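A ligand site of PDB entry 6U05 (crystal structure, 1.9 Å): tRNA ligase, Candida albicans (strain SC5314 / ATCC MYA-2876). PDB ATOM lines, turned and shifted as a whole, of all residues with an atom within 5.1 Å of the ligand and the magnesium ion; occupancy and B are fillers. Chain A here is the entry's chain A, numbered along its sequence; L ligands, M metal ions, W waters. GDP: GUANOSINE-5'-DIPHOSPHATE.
The magnesium ion is bound by the side-chain hydroxyl (OG1) of Thr 26 (2.1 Å), water W5 (2.1 Å), an oxygen (O1B) of the ligand (2.1 Å), water W9 (2.2 Å), water W7 (2.2 Å) and water W3 (2.3 Å).
The magnesium ion has six donor atoms within binding distance.
The backbone NH (N) of Thr 26 is in hydrogen-bond range of an oxygen (O1A) of the ligand (3.3 Å).
O6 of the ligand sits at hydrogen-bond distance from N of Ser 190 (2.7 Å).
OG of Ser 190 is in hydrogen-bond range of N7 of the ligand.
O1A of the ligand is in hydrogen-bond range of N of Thr 27, 2.7 Å away.
O1A of the ligand is in hydrogen-bond range of OG1 of Thr 27 (2.5 Å).
The side-chain carboxylate of Asp 183 is in hydrogen-bond range of a nitrogen (N1) of the ligand (2.7 Å).
The backbone NH (N) of Lys 25 sits at hydrogen-bond distance from an oxygen (O2B) of the ligand, 2.9 Å away.
An oxygen (O2B) of the ligand is in salt-bridge range of the side-chain amino group of Lys 25.
The backbone NH of Gly 22 sits at hydrogen-bond distance from an oxygen (O3B) of the ligand.
O6 of the ligand is in hydrogen-bond range of N of Ser 189 (3.2 Å).
The side-chain hydroxyl (OG) of Ser 189 lies within hydrogen-bond range of an oxygen (O6) of the ligand, 3.5 Å away.
The backbone NH (N) of Gly 24 sits at hydrogen-bond distance from an oxygen (O2B) of the ligand (3.2 Å).
N3 of the ligand sits close to NE of Arg 128.
The backbone NH (N) of Cys 23 lies within hydrogen-bond range of an oxygen (O2B) of the ligand, at 3.4 Å.
Residues that only touch the ligand: Lys 188 (3.4 Å), Leu 226 (3.7 Å) and Ile 21 (3.8 Å).
Hydrophobic or aromatic side chains within 4 Å of the ligand: Leu 226.
13 residues have an atom within 4 Å of the ligand: Ile 21, Gly 22, Cys 23, Gly 24, Lys 25, Thr 26, Thr 27, Arg 128, Asp 183, Lys 188, Ser 189, Ser 190 and Leu 226.
The nearest printed residue that does not touch the ligand is Thr 20 (4.1 Å).
Water W7 lies within hydrogen-bond range of an oxygen (O2A) of the ligand and the backbone carbonyl oxygen of Thr 231.
Water W9 lies within hydrogen-bond range of the side-chain carboxylate of Asp 45 (2.6 Å), an oxygen (O3B) of the ligand (3.0 Å) and the backbone carbonyl oxygen of Thr 231 (3.1 Å).
Water W1 lies within hydrogen-bond range of an oxygen (O3B) of the ligand and the backbone carbonyl oxygen of Thr 231.
Water W8 lies within hydrogen-bond range of the side-chain amino group (NZ) of Lys 25, an oxygen (O3B) of the ligand and the side-chain amide nitrogen (ND2) of Asn 76.
Water W6 lies within hydrogen-bond range of O of Gly 22 (2.7 Å), NH1 of Arg 128 (2.9 Å), O4' of the ligand (3.0 Å) and N of Gly 24 (3.1 Å).
Water W2 lies within hydrogen-bond range of O of Leu 226 (3.0 Å), OG1 of Thr 27 (3.3 Å) and O2' of the ligand (3.4 Å).
Residues that only touch the magnesium ion: Asp 45 (3.7 Å) and Thr 231 (3.8 Å).
Within 4 Å of the magnesium ion: Thr 26, Asp 45 and Thr 231.
Along chain A the residues within 4 Å of the magnesium ion span positions 26 to 231.
The side-chain carboxylate of Asp 74 lies close to the side-chain hydroxyl of Thr 26 (2.8 Å).
OD2 of Asp 183 lies within hydrogen-bond range of N of Ser 189, 2.9 Å away.
NZ of Lys 188 lies within salt-bridge range of OD1 of Asp 183 (3.4 Å).
The backbone carbonyl oxygen (O) of Thr 20 is in hydrogen-bond range of the side-chain amino group (NZ) of Lys 25, at 3.4 Å.
The side-chain amino group (NZ) of Lys 25 sits at hydrogen-bond distance from the side-chain amide oxygen (OD1) of Asn 76, 2.7 Å away.
The guanidinium group of Arg 128 is in hydrogen-bond range of the side-chain hydroxyl of Ser 189, at 2.7 Å.
The backbone carbonyl oxygen of Thr 20 sits at hydrogen-bond distance from the side-chain sulfur of Cys 23 (3.4 Å).
The backbone NH (N) of Ile 21 sits at hydrogen-bond distance from the side-chain amide oxygen (OD1) of Asn 76 (3.5 Å).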
ATOM      1  N   THR A  20       4.519  27.858  -0.877  1.00  0.00           N
ATOM      2  CA  THR A  20       4.128  27.766  -2.271  1.00  0.00           C
ATOM      3  C   THR A  20       2.603  27.639  -2.327  1.00  0.00           C
ATOM      4  O   THR A  20       1.923  27.683  -1.298  1.00  0.00           O
ATOM      5  CB  THR A  20       4.839  26.593  -2.960  1.00  0.00           C
ATOM      6  OG1 THR A  20       4.559  25.363  -2.266  1.00  0.00           O
ATOM      7  CG2 THR A  20       6.345  26.847  -2.969  1.00  0.00           C
ATOM      8  N   ILE A  21       2.077  27.517  -3.545  1.00  0.00           N
ATOM      9  CA  ILE A  21       0.628  27.491  -3.716  1.00  0.00           C
ATOM     10  C   ILE A  21       0.032  26.238  -3.089  1.00  0.00           C
ATOM     11  O   ILE A  21       0.565  25.126  -3.242  1.00  0.00           O
ATOM     12  CB  ILE A  21       0.280  27.588  -5.217  1.00  0.00           C
ATOM     13  CG1 ILE A  21       0.601  28.972  -5.772  1.00  0.00           C
ATOM     14  CG2 ILE A  21      -1.196  27.253  -5.460  1.00  0.00           C
ATOM     15  CD1 ILE A  21       0.396  29.045  -7.281  1.00  0.00           C
ATOM     16  N   GLY A  22      -1.091  26.398  -2.393  1.00  0.00           N
ATOM     17  CA  GLY A  22      -1.839  25.268  -1.907  1.00  0.00           C
ATOM     18  C   GLY A  22      -1.375  24.711  -0.581  1.00  0.00           C
ATOM     19  O   GLY A  22      -1.841  23.645  -0.166  1.00  0.00           O
ATOM     20  N   CYS A  23      -0.459  25.405   0.091  1.00  0.00           N
ATOM     21  CA  CYS A  23       0.024  25.017   1.405  1.00  0.00           C
ATOM     22  C   CYS A  23      -0.991  25.277   2.496  1.00  0.00           C
ATOM     23  O   CYS A  23      -0.745  24.881   3.646  1.00  0.00           O
ATOM     24  CB  CYS A  23       1.333  25.744   1.716  1.00  0.00           C
ATOM     25  SG  CYS A  23       2.814  25.114   0.764  1.00  0.00           S
ATOM     26  N   GLY A  24      -2.094  25.955   2.185  1.00  0.00           N
ATOM     27  CA  GLY A  24      -3.080  26.292   3.186  1.00  0.00           C
ATOM     28  C   GLY A  24      -2.987  27.688   3.748  1.00  0.00           C
ATOM     29  O   GLY A  24      -3.646  27.966   4.760  1.00  0.00           O
ATOM     30  N   LYS A  25      -2.221  28.593   3.114  1.00  0.00           N
ATOM     31  CA  LYS A  25      -2.100  29.959   3.600  1.00  0.00           C
ATOM     32  C   LYS A  25      -3.456  30.610   3.814  1.00  0.00           C
ATOM     33  O   LYS A  25      -3.743  31.181   4.883  1.00  0.00           O
ATOM     34  CB  LYS A  25      -1.288  30.817   2.614  1.00  0.00           C
ATOM     35  CG  LYS A  25       0.191  30.535   2.528  1.00  0.00           C
ATOM     36  CD  LYS A  25       0.886  31.468   1.534  1.00  0.00           C
ATOM     37  CE  LYS A  25       0.103  31.650   0.228  1.00  0.00           C
ATOM     38  NZ  LYS A  25       0.012  30.386  -0.546  1.00  0.00           N
ATOM     39  N   THR A  26      -4.295  30.604   2.773  1.00  0.00           N
ATOM     40  CA  THR A  26      -5.534  31.347   2.875  1.00  0.00           C
ATOM     41  C   THR A  26      -6.495  30.686   3.846  1.00  0.00           C
ATOM     42  O   THR A  26      -7.215  31.363   4.580  1.00  0.00           O
ATOM     43  CB  THR A  26      -6.127  31.508   1.480  1.00  0.00           C
ATOM     44  OG1 THR A  26      -5.158  32.193   0.654  1.00  0.00           O
ATOM     45  CG2 THR A  26      -7.445  32.281   1.520  1.00  0.00           C
ATOM     46  N   THR A  27      -6.502  29.344   3.866  1.00  0.00           N
ATOM     47  CA  THR A  27      -7.306  28.612   4.829  1.00  0.00           C
ATOM     48  C   THR A  27      -6.905  28.947   6.261  1.00  0.00           C
ATOM     49  O   THR A  27      -7.764  29.196   7.115  1.00  0.00           O
ATOM     50  CB  THR A  27      -7.151  27.115   4.573  1.00  0.00           C
ATOM     51  OG1 THR A  27      -7.553  26.848   3.219  1.00  0.00           O
ATOM     52  CG2 THR A  27      -8.001  26.313   5.540  1.00  0.00           C
ATOM     53  N   VAL A  28      -5.605  28.909   6.549  1.00  0.00           N
ATOM     54  CA  VAL A  28      -5.134  29.198   7.903  1.00  0.00           C
ATOM     55  C   VAL A  28      -5.461  30.650   8.262  1.00  0.00           C
ATOM     56  O   VAL A  28      -5.990  30.952   9.337  1.00  0.00           O
ATOM     57  CB  VAL A  28      -3.637  28.880   8.018  1.00  0.00           C
ATOM     58  CG1 VAL A  28      -3.030  29.507   9.279  1.00  0.00           C
ATOM     59  CG2 VAL A  28      -3.380  27.377   8.007  1.00  0.00           C
ATOM     60  N   GLN A  43      -5.145  39.669   0.820  1.00  0.00           N
ATOM     61  CA  GLN A  43      -4.826  38.577  -0.105  1.00  0.00           C
ATOM     62  C   GLN A  43      -4.241  39.140  -1.384  1.00  0.00           C
ATOM     63  O   GLN A  43      -4.920  39.866  -2.125  1.00  0.00           O
ATOM     64  CB  GLN A  43      -6.071  37.742  -0.422  1.00  0.00           C
ATOM     65  CG  GLN A  43      -6.631  37.020   0.792  1.00  0.00           C
ATOM     66  CD  GLN A  43      -7.701  36.013   0.440  1.00  0.00           C
ATOM     67  OE1 GLN A  43      -7.510  35.146  -0.412  1.00  0.00           O
ATOM     68  NE2 GLN A  43      -8.849  36.122   1.098  1.00  0.00           N
ATOM     69  N   ASP A  45      -3.678  37.596  -4.026  1.00  0.00           N
ATOM     70  CA  ASP A  45      -4.416  37.090  -5.170  1.00  0.00           C
ATOM     71  C   ASP A  45      -5.530  38.026  -5.594  1.00  0.00           C
ATOM     72  O   ASP A  45      -5.958  37.999  -6.752  1.00  0.00           O
ATOM     73  CB  ASP A  45      -5.039  35.716  -4.855  1.00  0.00           C
ATOM     74  CG  ASP A  45      -4.012  34.615  -4.797  1.00  0.00           C
ATOM     75  OD1 ASP A  45      -2.847  34.854  -5.194  1.00  0.00           O
ATOM     76  OD2 ASP A  45      -4.372  33.492  -4.366  1.00  0.00           O
ATOM     77  N   ASP A  74      -1.085  37.831   3.014  1.00  0.00           N
ATOM     78  CA  ASP A  74      -1.354  36.572   2.322  1.00  0.00           C
ATOM     79  C   ASP A  74      -0.692  36.568   0.944  1.00  0.00           C
ATOM     80  O   ASP A  74      -1.299  36.909  -0.076  1.00  0.00           O
ATOM     81  CB  ASP A  74      -2.854  36.333   2.221  1.00  0.00           C
ATOM     82  CG  ASP A  74      -3.193  34.884   1.828  1.00  0.00           C
ATOM     83  OD1 ASP A  74      -2.291  34.171   1.345  1.00  0.00           O
ATOM     84  OD2 ASP A  74      -4.361  34.482   2.018  1.00  0.00           O
ATOM     85  N   ASN A  76       2.834  34.274  -1.132  1.00  0.00           N
ATOM     86  CA  ASN A  76       3.689  33.084  -1.015  1.00  0.00           C
ATOM     87  C   ASN A  76       5.073  33.416  -0.484  1.00  0.00           C
ATOM     88  O   ASN A  76       5.596  32.719   0.398  1.00  0.00           O
ATOM     89  CB  ASN A  76       3.804  32.390  -2.369  1.00  0.00           C
ATOM     90  CG  ASN A  76       2.658  31.432  -2.629  1.00  0.00           C
ATOM     91  OD1 ASN A  76       2.399  30.521  -1.845  1.00  0.00           O
ATOM     92  ND2 ASN A  76       1.946  31.654  -3.728  1.00  0.00           N
ATOM     93  N   ARG A 128      -4.271  18.844  -3.508  1.00  0.00           N
ATOM     94  CA  ARG A 128      -5.199  19.717  -2.781  1.00  0.00           C
ATOM     95  C   ARG A 128      -5.872  20.723  -3.717  1.00  0.00           C
ATOM     96  O   ARG A 128      -7.067  20.996  -3.577  1.00  0.00           O
ATOM     97  CB  ARG A 128      -4.458  20.459  -1.661  1.00  0.00           C
ATOM     98  CG  ARG A 128      -4.361  19.636  -0.396  1.00  0.00           C
ATOM     99  CD  ARG A 128      -3.745  20.411   0.721  1.00  0.00           C
ATOM    100  NE  ARG A 128      -3.355  19.544   1.825  1.00  0.00           N
ATOM    101  CZ  ARG A 128      -2.809  20.006   2.941  1.00  0.00           C
ATOM    102  NH1 ARG A 128      -2.634  21.303   3.075  1.00  0.00           N
ATOM    103  NH2 ARG A 128      -2.470  19.177   3.924  1.00  0.00           N
ATOM    104  N   VAL A 129      -5.131  21.272  -4.675  1.00  0.00           N
ATOM    105  CA  VAL A 129      -5.671  22.349  -5.510  1.00  0.00           C
ATOM    106  C   VAL A 129      -6.730  21.811  -6.459  1.00  0.00           C
ATOM    107  O   VAL A 129      -7.789  22.431  -6.639  1.00  0.00           O
ATOM    108  CB  VAL A 129      -4.531  23.059  -6.264  1.00  0.00           C
ATOM    109  CG1 VAL A 129      -5.104  24.066  -7.254  1.00  0.00           C
ATOM    110  CG2 VAL A 129      -3.592  23.752  -5.264  1.00  0.00           C
ATOM    111  N   ASP A 183      -3.367  14.182   4.905  1.00  0.00           N
ATOM    112  CA  ASP A 183      -4.043  14.134   6.196  1.00  0.00           C
ATOM    113  C   ASP A 183      -5.429  13.516   6.103  1.00  0.00           C
ATOM    114  O   ASP A 183      -6.315  13.850   6.897  1.00  0.00           O
ATOM    115  CB  ASP A 183      -4.167  15.531   6.803  1.00  0.00           C
ATOM    116  CG  ASP A 183      -4.670  16.564   5.789  1.00  0.00           C
ATOM    117  OD1 ASP A 183      -5.297  16.154   4.778  1.00  0.00           O
ATOM    118  OD2 ASP A 183      -4.438  17.785   5.993  1.00  0.00           O
ATOM    119  N   LYS A 188      -6.622  17.588  10.108  1.00  0.00           N
ATOM    120  CA  LYS A 188      -6.129  18.324   8.951  1.00  0.00           C
ATOM    121  C   LYS A 188      -4.916  19.153   9.341  1.00  0.00           C
ATOM    122  O   LYS A 188      -4.864  19.716  10.440  1.00  0.00           O
ATOM    123  CB  LYS A 188      -7.225  19.213   8.366  1.00  0.00           C
ATOM    124  CG  LYS A 188      -8.415  18.416   7.807  1.00  0.00           C
ATOM    125  CD  LYS A 188      -8.555  18.621   6.296  1.00  0.00           C
ATOM    126  CE  LYS A 188      -9.341  17.481   5.645  1.00  0.00           C
ATOM    127  NZ  LYS A 188      -8.584  16.170   5.615  1.00  0.00           N
ATOM    128  N   SER A 189      -3.924  19.221   8.445  1.00  0.00           N
ATOM    129  CA  SER A 189      -2.719  19.941   8.816  1.00  0.00           C
ATOM    130  C   SER A 189      -2.962  21.440   8.997  1.00  0.00           C
ATOM    131  O   SER A 189      -2.325  22.054   9.854  1.00  0.00           O
ATOM    132  CB  SER A 189      -1.566  19.678   7.812  1.00  0.00           C
ATOM    133  OG  SER A 189      -1.913  19.916   6.460  1.00  0.00           O
ATOM    134  N   SER A 190      -3.916  22.049   8.264  1.00  0.00           N
ATOM    135  CA  SER A 190      -4.165  23.473   8.535  1.00  0.00           C
ATOM    136  C   SER A 190      -4.830  23.686   9.892  1.00  0.00           C
ATOM    137  O   SER A 190      -4.659  24.739  10.510  1.00  0.00           O
ATOM    138  CB  SER A 190      -5.022  24.133   7.442  1.00  0.00           C
ATOM    139  OG  SER A 190      -4.523  23.860   6.139  1.00  0.00           O
ATOM    140  N   LEU A 191      -5.585  22.690  10.394  1.00  0.00           N
ATOM    141  CA  LEU A 191      -6.182  22.877  11.714  1.00  0.00           C
ATOM    142  C   LEU A 191      -5.136  22.722  12.801  1.00  0.00           C
ATOM    143  O   LEU A 191      -5.132  23.483  13.777  1.00  0.00           O
ATOM    144  CB  LEU A 191      -7.337  21.892  11.922  1.00  0.00           C
ATOM    145  CG  LEU A 191      -8.058  21.941  13.276  1.00  0.00           C
ATOM    146  CD1 LEU A 191      -8.422  23.364  13.633  1.00  0.00           C
ATOM    147  CD2 LEU A 191      -9.316  21.072  13.255  1.00  0.00           C
ATOM    148  N   PHE A 222     -12.546  26.933  11.744  1.00  0.00           N
ATOM    149  CA  PHE A 222     -11.766  26.257  10.716  1.00  0.00           C
ATOM    150  C   PHE A 222     -12.668  25.596   9.693  1.00  0.00           C
ATOM    151  O   PHE A 222     -12.409  25.676   8.484  1.00  0.00           O
ATOM    152  CB  PHE A 222     -10.837  25.242  11.361  1.00  0.00           C
ATOM    153  CG  PHE A 222     -10.170  24.354  10.369  1.00  0.00           C
ATOM    154  CD1 PHE A 222      -9.093  24.830   9.623  1.00  0.00           C
ATOM    155  CD2 PHE A 222     -10.610  23.058  10.160  1.00  0.00           C
ATOM    156  CE1 PHE A 222      -8.472  24.039   8.694  1.00  0.00           C
ATOM    157  CE2 PHE A 222      -9.992  22.254   9.233  1.00  0.00           C
ATOM    158  CZ  PHE A 222      -8.928  22.734   8.496  1.00  0.00           C
ATOM    159  N   LEU A 226     -12.452  26.076   5.902  1.00  0.00           N
ATOM    160  CA  LEU A 226     -12.211  24.960   4.997  1.00  0.00           C
ATOM    161  C   LEU A 226     -13.237  24.924   3.872  1.00  0.00           C
ATOM    162  O   LEU A 226     -12.896  24.546   2.745  1.00  0.00           O
ATOM    163  CB  LEU A 226     -12.201  23.629   5.774  1.00  0.00           C
ATOM    164  CG  LEU A 226     -11.583  22.410   5.080  1.00  0.00           C
ATOM    165  CD1 LEU A 226     -10.102  22.590   4.798  1.00  0.00           C
ATOM    166  CD2 LEU A 226     -11.836  21.116   5.891  1.00  0.00           C
ATOM    167  N   PRO A 230     -12.507  28.951  -2.770  1.00  0.00           N
ATOM    168  CA  PRO A 230     -11.052  29.158  -2.828  1.00  0.00           C
ATOM    169  C   PRO A 230     -10.689  30.341  -3.704  1.00  0.00           C
ATOM    170  O   PRO A 230     -11.459  30.802  -4.558  1.00  0.00           O
ATOM    171  CB  PRO A 230     -10.547  27.848  -3.447  1.00  0.00           C
ATOM    172  CG  PRO A 230     -11.710  27.311  -4.204  1.00  0.00           C
ATOM    173  CD  PRO A 230     -12.903  27.677  -3.377  1.00  0.00           C
ATOM    174  N   THR A 231      -9.477  30.844  -3.478  1.00  0.00           N
ATOM    175  CA  THR A 231      -8.903  31.940  -4.237  1.00  0.00           C
ATOM    176  C   THR A 231      -7.600  31.439  -4.859  1.00  0.00           C
ATOM    177  O   THR A 231      -6.755  30.877  -4.164  1.00  0.00           O
ATOM    178  CB  THR A 231      -8.620  33.162  -3.361  1.00  0.00           C
ATOM    179  OG1 THR A 231      -9.723  33.372  -2.466  1.00  0.00           O
ATOM    180  CG2 THR A 231      -8.418  34.397  -4.204  1.00  0.00           C
HETATM  181  PB  GDP L   1      -3.048  28.653  -0.526  1.00  0.00           P
HETATM  182  O1B GDP L   1      -3.828  29.854  -0.127  1.00  0.00           O
HETATM  183  O2B GDP L   1      -1.756  28.541   0.262  1.00  0.00           O
HETATM  184  O3B GDP L   1      -2.765  28.598  -2.015  1.00  0.00           O
HETATM  185  O3A GDP L   1      -3.918  27.334  -0.128  1.00  0.00           O
HETATM  186  PA  GDP L   1      -5.442  27.388   0.337  1.00  0.00           P
HETATM  187  O1A GDP L   1      -5.723  27.842   1.759  1.00  0.00           O
HETATM  188  O2A GDP L   1      -6.255  28.191  -0.652  1.00  0.00           O
HETATM  189  O5' GDP L   1      -5.862  25.830   0.268  1.00  0.00           O
HETATM  190  C5' GDP L   1      -5.818  25.147  -0.992  1.00  0.00           C
HETATM  191  C4' GDP L   1      -6.780  23.953  -0.974  1.00  0.00           C
HETATM  192  O4' GDP L   1      -6.401  23.073   0.074  1.00  0.00           O
HETATM  193  C3' GDP L   1      -8.202  24.377  -0.639  1.00  0.00           C
HETATM  194  O3' GDP L   1      -9.120  23.551  -1.331  1.00  0.00           O
HETATM  195  C2' GDP L   1      -8.363  24.069   0.819  1.00  0.00           C
HETATM  196  O2' GDP L   1      -9.703  23.757   1.162  1.00  0.00           O
HETATM  197  C1' GDP L   1      -7.495  22.849   0.947  1.00  0.00           C
HETATM  198  N9  GDP L   1      -6.957  22.740   2.310  1.00  0.00           N
HETATM  199  C8  GDP L   1      -6.673  23.739   3.155  1.00  0.00           C
HETATM  200  N7  GDP L   1      -6.159  23.245   4.309  1.00  0.00           N
HETATM  201  C5  GDP L   1      -6.116  21.896   4.187  1.00  0.00           C
HETATM  202  C6  GDP L   1      -5.681  20.760   5.017  1.00  0.00           C
HETATM  203  O6  GDP L   1      -5.224  20.984   6.177  1.00  0.00           O
HETATM  204  N1  GDP L   1      -5.799  19.514   4.515  1.00  0.00           N
HETATM  205  C2  GDP L   1      -6.289  19.279   3.273  1.00  0.00           C
HETATM  206  N2  GDP L   1      -6.376  17.996   2.815  1.00  0.00           N
HETATM  207  N3  GDP L   1      -6.693  20.280   2.454  1.00  0.00           N
HETATM  208  C4  GDP L   1      -6.633  21.576   2.852  1.00  0.00           C
HETATM  209 MG    MG M   1      -4.478  31.582  -1.188  1.00  0.00          MG
HETATM  210  O   HOH W   1      -4.477  28.578  -4.093  1.00  0.00           O
HETATM  211  O   HOH W   2     -10.760  26.684   2.512  1.00  0.00           O
HETATM  212  O   HOH W   3      -5.736  33.482  -1.699  1.00  0.00           O
HETATM  213  O   HOH W   4     -11.188  21.481   0.909  1.00  0.00           O
HETATM  214  O   HOH W   5      -2.717  32.670  -0.903  1.00  0.00           O
HETATM  215  O   HOH W   6      -3.826  23.475   1.642  1.00  0.00           O
HETATM  216  O   HOH W   7      -6.410  30.555  -1.616  1.00  0.00           O
HETATM  217  O   HOH W   8      -0.925  30.667  -2.834  1.00  0.00           O
HETATM  218  O   HOH W   9      -3.766  31.194  -3.227  1.00  0.00           O
